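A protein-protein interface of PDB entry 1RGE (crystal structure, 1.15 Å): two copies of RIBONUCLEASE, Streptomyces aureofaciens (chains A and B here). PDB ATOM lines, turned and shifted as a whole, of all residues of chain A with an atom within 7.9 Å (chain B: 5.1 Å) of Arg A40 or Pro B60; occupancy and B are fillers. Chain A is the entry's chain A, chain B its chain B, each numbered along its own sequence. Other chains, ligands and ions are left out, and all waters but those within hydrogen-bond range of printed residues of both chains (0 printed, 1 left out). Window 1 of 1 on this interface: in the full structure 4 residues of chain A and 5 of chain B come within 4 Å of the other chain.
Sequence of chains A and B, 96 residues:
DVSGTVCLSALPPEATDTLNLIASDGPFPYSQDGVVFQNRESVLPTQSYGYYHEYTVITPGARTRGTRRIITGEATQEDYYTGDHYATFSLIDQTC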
ATOM      1  N   VAL A  36     -22.847 -18.511 -22.764  1.00  0.00           N
ATOM      2  CA  VAL A  36     -21.604 -18.536 -23.525  1.00  0.00           C
ATOM      3  C   VAL A  36     -20.476 -19.126 -22.657  1.00  0.00           C
ATOM      4  O   VAL A  36     -20.325 -18.768 -21.484  1.00  0.00           O
ATOM      5  CB  VAL A  36     -21.249 -17.108 -24.009  1.00  0.00           C
ATOM      6  CG1 VAL A  36     -19.838 -17.076 -24.588  1.00  0.00           C
ATOM      7  CG2 VAL A  36     -22.236 -16.656 -25.053  1.00  0.00           C
ATOM      8  N   PHE A  37     -19.659 -19.968 -23.275  1.00  0.00           N
ATOM      9  CA  PHE A  37     -18.415 -20.412 -22.697  1.00  0.00           C
ATOM     10  C   PHE A  37     -17.302 -19.554 -23.310  1.00  0.00           C
ATOM     11  O   PHE A  37     -17.171 -19.487 -24.512  1.00  0.00           O
ATOM     12  CB  PHE A  37     -18.183 -21.873 -22.997  1.00  0.00           C
ATOM     13  CG  PHE A  37     -16.884 -22.411 -22.484  1.00  0.00           C
ATOM     14  CD1 PHE A  37     -16.712 -22.580 -21.133  1.00  0.00           C
ATOM     15  CD2 PHE A  37     -15.858 -22.707 -23.373  1.00  0.00           C
ATOM     16  CE1 PHE A  37     -15.477 -23.039 -20.655  1.00  0.00           C
ATOM     17  CE2 PHE A  37     -14.656 -23.169 -22.878  1.00  0.00           C
ATOM     18  CZ  PHE A  37     -14.459 -23.325 -21.523  1.00  0.00           C
ATOM     19  N   GLN A  38     -16.540 -18.879 -22.437  1.00  0.00           N
ATOM     20  CA  GLN A  38     -15.581 -17.899 -22.897  1.00  0.00           C
ATOM     21  C   GLN A  38     -14.334 -18.455 -23.514  1.00  0.00           C
ATOM     22  O   GLN A  38     -13.610 -17.735 -24.213  1.00  0.00           O
ATOM     23  CB  GLN A  38     -15.202 -16.942 -21.771  1.00  0.00           C
ATOM     24  CG  GLN A  38     -16.287 -16.023 -21.302  1.00  0.00           C
ATOM     25  CD  GLN A  38     -15.611 -14.922 -20.450  1.00  0.00           C
ATOM     26  OE1 GLN A  38     -14.494 -14.402 -20.732  1.00  0.00           O
ATOM     27  NE2 GLN A  38     -16.310 -14.518 -19.468  1.00  0.00           N
ATOM     28  N   ASN A  39     -14.010 -19.720 -23.210  1.00  0.00           N
ATOM     29  CA  ASN A  39     -12.710 -20.256 -23.594  1.00  0.00           C
ATOM     30  C   ASN A  39     -11.562 -19.415 -23.078  1.00  0.00           C
ATOM     31  O   ASN A  39     -10.548 -19.203 -23.775  1.00  0.00           O
ATOM     32  CB  ASN A  39     -12.611 -20.496 -25.074  1.00  0.00           C
ATOM     33  CG  ASN A  39     -11.478 -21.355 -25.496  1.00  0.00           C
ATOM     34  OD1 ASN A  39     -11.090 -22.289 -24.810  1.00  0.00           O
ATOM     35  ND2 ASN A  39     -10.948 -21.071 -26.705  1.00  0.00           N
ATOM     36  N   ARG A  40     -11.669 -18.967 -21.857  1.00  0.00           N
ATOM     37  CA  ARG A  40     -10.726 -17.996 -21.295  1.00  0.00           C
ATOM     38  C   ARG A  40      -9.349 -18.563 -21.206  1.00  0.00           C
ATOM     39  O   ARG A  40      -8.349 -17.800 -21.330  1.00  0.00           O
ATOM     40  CB  ARG A  40     -11.209 -17.505 -19.938  1.00  0.00           C
ATOM     41  CG  ARG A  40     -10.530 -16.356 -19.283  1.00  0.00           C
ATOM     42  CD  ARG A  40     -11.187 -16.368 -17.839  1.00  0.00           C
ATOM     43  NE  ARG A  40     -12.518 -15.835 -17.987  1.00  0.00           N
ATOM     44  CZ  ARG A  40     -13.553 -16.208 -17.217  1.00  0.00           C
ATOM     45  NH1 ARG A  40     -13.390 -16.825 -16.049  1.00  0.00           N
ATOM     46  NH2 ARG A  40     -14.782 -15.881 -17.586  1.00  0.00           N
ATOM     47  N   GLU A  41      -9.221 -19.832 -20.914  1.00  0.00           N
ATOM     48  CA  GLU A  41      -7.965 -20.516 -20.716  1.00  0.00           C
ATOM     49  C   GLU A  41      -7.316 -20.957 -22.011  1.00  0.00           C
ATOM     50  O   GLU A  41      -6.219 -21.459 -22.002  1.00  0.00           O
ATOM     51  CB  GLU A  41      -8.105 -21.678 -19.742  1.00  0.00           C
ATOM     52  CG  GLU A  41      -8.557 -21.304 -18.351  1.00  0.00           C
ATOM     53  CD  GLU A  41      -9.976 -20.878 -18.190  1.00  0.00           C
ATOM     54  OE1 GLU A  41     -10.910 -21.391 -18.803  1.00  0.00           O
ATOM     55  OE2 GLU A  41     -10.124 -19.874 -17.443  1.00  0.00           O
ATOM     56  N   SER A  42      -7.994 -20.722 -23.158  1.00  0.00           N
ATOM     57  CA  SER A  42      -7.469 -21.077 -24.443  1.00  0.00           C
ATOM     58  C   SER A  42      -7.193 -22.544 -24.605  1.00  0.00           C
ATOM     59  O   SER A  42      -6.293 -22.950 -25.333  1.00  0.00           O
ATOM     60  CB  SER A  42      -6.237 -20.220 -24.817  1.00  0.00           C
ATOM     61  OG  SER A  42      -6.067 -20.245 -26.212  1.00  0.00           O
ATOM     62  N   VAL A  43      -7.995 -23.394 -23.944  1.00  0.00           N
ATOM     63  CA  VAL A  43      -7.852 -24.836 -24.104  1.00  0.00           C
ATOM     64  C   VAL A  43      -8.430 -25.278 -25.467  1.00  0.00           C
ATOM     65  O   VAL A  43      -7.879 -26.143 -26.101  1.00  0.00           O
ATOM     66  CB  VAL A  43      -8.469 -25.612 -22.952  1.00  0.00           C
ATOM     67  CG1 VAL A  43      -8.266 -27.112 -23.105  1.00  0.00           C
ATOM     68  CG2 VAL A  43      -7.861 -25.163 -21.611  1.00  0.00           C
ATOM     69  N   LEU A  44      -9.541 -24.657 -25.842  1.00  0.00           N
ATOM     70  CA  LEU A  44     -10.169 -24.972 -27.125  1.00  0.00           C
ATOM     71  C   LEU A  44      -9.638 -24.044 -28.193  1.00  0.00           C
ATOM     72  O   LEU A  44      -9.055 -22.998 -27.858  1.00  0.00           O
ATOM     73  CB  LEU A  44     -11.697 -24.845 -27.024  1.00  0.00           C
ATOM     74  CG  LEU A  44     -12.373 -25.791 -26.014  1.00  0.00           C
ATOM     75  CD1 LEU A  44     -13.855 -25.518 -25.943  1.00  0.00           C
ATOM     76  CD2 LEU A  44     -12.084 -27.265 -26.368  1.00  0.00           C
ATOM     77  N   TYR A  52     -18.810 -20.567 -28.584  1.00  0.00           N
ATOM     78  CA  TYR A  52     -18.974 -21.700 -27.697  1.00  0.00           C
ATOM     79  C   TYR A  52     -20.055 -21.426 -26.677  1.00  0.00           C
ATOM     80  O   TYR A  52     -20.189 -20.312 -26.158  1.00  0.00           O
ATOM     81  CB  TYR A  52     -17.659 -21.990 -26.942  1.00  0.00           C
ATOM     82  CG  TYR A  52     -16.477 -22.351 -27.777  1.00  0.00           C
ATOM     83  CD1 TYR A  52     -16.390 -23.580 -28.449  1.00  0.00           C
ATOM     84  CD2 TYR A  52     -15.385 -21.515 -27.882  1.00  0.00           C
ATOM     85  CE1 TYR A  52     -15.297 -23.907 -29.190  1.00  0.00           C
ATOM     86  CE2 TYR A  52     -14.265 -21.846 -28.607  1.00  0.00           C
ATOM     87  CZ  TYR A  52     -14.223 -23.050 -29.273  1.00  0.00           C
ATOM     88  OH  TYR A  52     -13.142 -23.464 -30.008  1.00  0.00           O
ATOM     89  N   GLU B  14       3.085 -21.671 -24.798  1.00  0.00           N
ATOM     90  CA  GLU B  14       2.440 -21.201 -26.033  1.00  0.00           C
ATOM     91  C   GLU B  14       3.450 -20.725 -27.057  1.00  0.00           C
ATOM     92  O   GLU B  14       3.133 -20.674 -28.242  1.00  0.00           O
ATOM     93  CB  GLU B  14       1.403 -20.113 -25.723  1.00  0.00           C
ATOM     94  CG  GLU B  14       0.277 -20.588 -24.803  1.00  0.00           C
ATOM     95  CD  GLU B  14       0.583 -20.749 -23.367  1.00  0.00           C
ATOM     96  OE1 GLU B  14       1.566 -20.137 -22.876  1.00  0.00           O
ATOM     97  OE2 GLU B  14      -0.139 -21.501 -22.680  1.00  0.00           O
ATOM     98  N   ILE B  58      -0.262 -16.874 -27.847  1.00  0.00           N
ATOM     99  CA  ILE B  58      -1.437 -16.708 -27.023  1.00  0.00           C
ATOM    100  C   ILE B  58      -1.056 -16.574 -25.564  1.00  0.00           C
ATOM    101  O   ILE B  58      -0.212 -17.314 -25.083  1.00  0.00           O
ATOM    102  CB  ILE B  58      -2.416 -17.860 -27.261  1.00  0.00           C
ATOM    103  CG1 ILE B  58      -2.979 -17.782 -28.702  1.00  0.00           C
ATOM    104  CG2 ILE B  58      -3.487 -17.937 -26.213  1.00  0.00           C
ATOM    105  CD1 ILE B  58      -3.749 -18.955 -29.133  1.00  0.00           C
ATOM    106  N   THR B  59      -1.731 -15.649 -24.873  1.00  0.00           N
ATOM    107  CA  THR B  59      -1.625 -15.517 -23.434  1.00  0.00           C
ATOM    108  C   THR B  59      -2.949 -16.038 -22.818  1.00  0.00           C
ATOM    109  O   THR B  59      -3.977 -15.414 -22.952  1.00  0.00           O
ATOM    110  CB  THR B  59      -1.458 -14.064 -23.007  1.00  0.00           C
ATOM    111  OG1 THR B  59      -0.222 -13.561 -23.587  1.00  0.00           O
ATOM    112  CG2 THR B  59      -1.308 -13.969 -21.525  1.00  0.00           C
ATOM    113  N   PRO B  60      -2.904 -17.231 -22.197  1.00  0.00           N
ATOM    114  CA  PRO B  60      -4.138 -17.709 -21.587  1.00  0.00           C
ATOM    115  C   PRO B  60      -4.633 -16.736 -20.532  1.00  0.00           C
ATOM    116  O   PRO B  60      -3.843 -16.141 -19.834  1.00  0.00           O
ATOM    117  CB  PRO B  60      -3.711 -19.029 -20.899  1.00  0.00           C
ATOM    118  CG  PRO B  60      -2.524 -19.473 -21.703  1.00  0.00           C
ATOM    119  CD  PRO B  60      -1.774 -18.170 -21.970  1.00  0.00           C
ATOM    120  N   GLY B  61      -5.942 -16.552 -20.518  1.00  0.00           N
ATOM    121  CA  GLY B  61      -6.543 -15.628 -19.546  1.00  0.00           C
ATOM    122  C   GLY B  61      -6.682 -14.225 -20.072  1.00  0.00           C
ATOM    123  O   GLY B  61      -7.467 -13.476 -19.503  1.00  0.00           O
ATOM    124  N   ALA B  62      -5.982 -13.837 -21.114  1.00  0.00           N
ATOM    125  CA  ALA B  62      -6.049 -12.492 -21.629  1.00  0.00           C
ATOM    126  C   ALA B  62      -7.308 -12.314 -22.460  1.00  0.00           C
ATOM    127  O   ALA B  62      -7.656 -13.203 -23.219  1.00  0.00           O
ATOM    128  CB  ALA B  62      -4.839 -12.137 -22.460  1.00  0.00           C
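The backbone carbonyl oxygen (O) of Arg A40 lies within hydrogen-bond range of the backbone NH (N) of Gly B61, at 2.8 Å.
The guanidinium group of Arg A40 lies close to the side-chain amide nitrogen of Gln A38.
Among the printed residues, pairs that only touch across the chains: Ser A42 with Ile B58 (3.5 Å), Glu A41 with Pro B60 (3.7 Å) and Arg A40 with Pro B60 (3.9 Å).
Of the 10 printed residues of chain A, 3 touch a printed residue of chain B. Among the printed residues, 4 pairs touch across the chains. Among the printed residues, no Asp or Glu carboxylate lies within 4 Å of a Lys or Arg side-chain nitrogen of the other chain.
Of the printed residues of chain B, Arg A40 touches Pro B60 (3.9 Å) and Gly B61 (2.8 Å). Of the printed residues of chain A, Pro B60 touches Arg A40 (3.9 Å) and Glu A41 (3.7 Å). Printed residues of chain B within 4 Å of Ser A42: Ile B58. Of the printed residues of chain B, Glu A41 touches Pro B60 (3.7 Å). Printed residues of chain A within 4 Å of Ile B58: Ser A42 (3.5 Å). Of the printed residues of chain A, Gly B61 touches Arg A40. Ala B62 touches none of the printed residues of chain A. The nearest printed residue of chain B that does not touch Arg A40 is Ala B62 (4.6 Å).
No position is printed for both chains.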
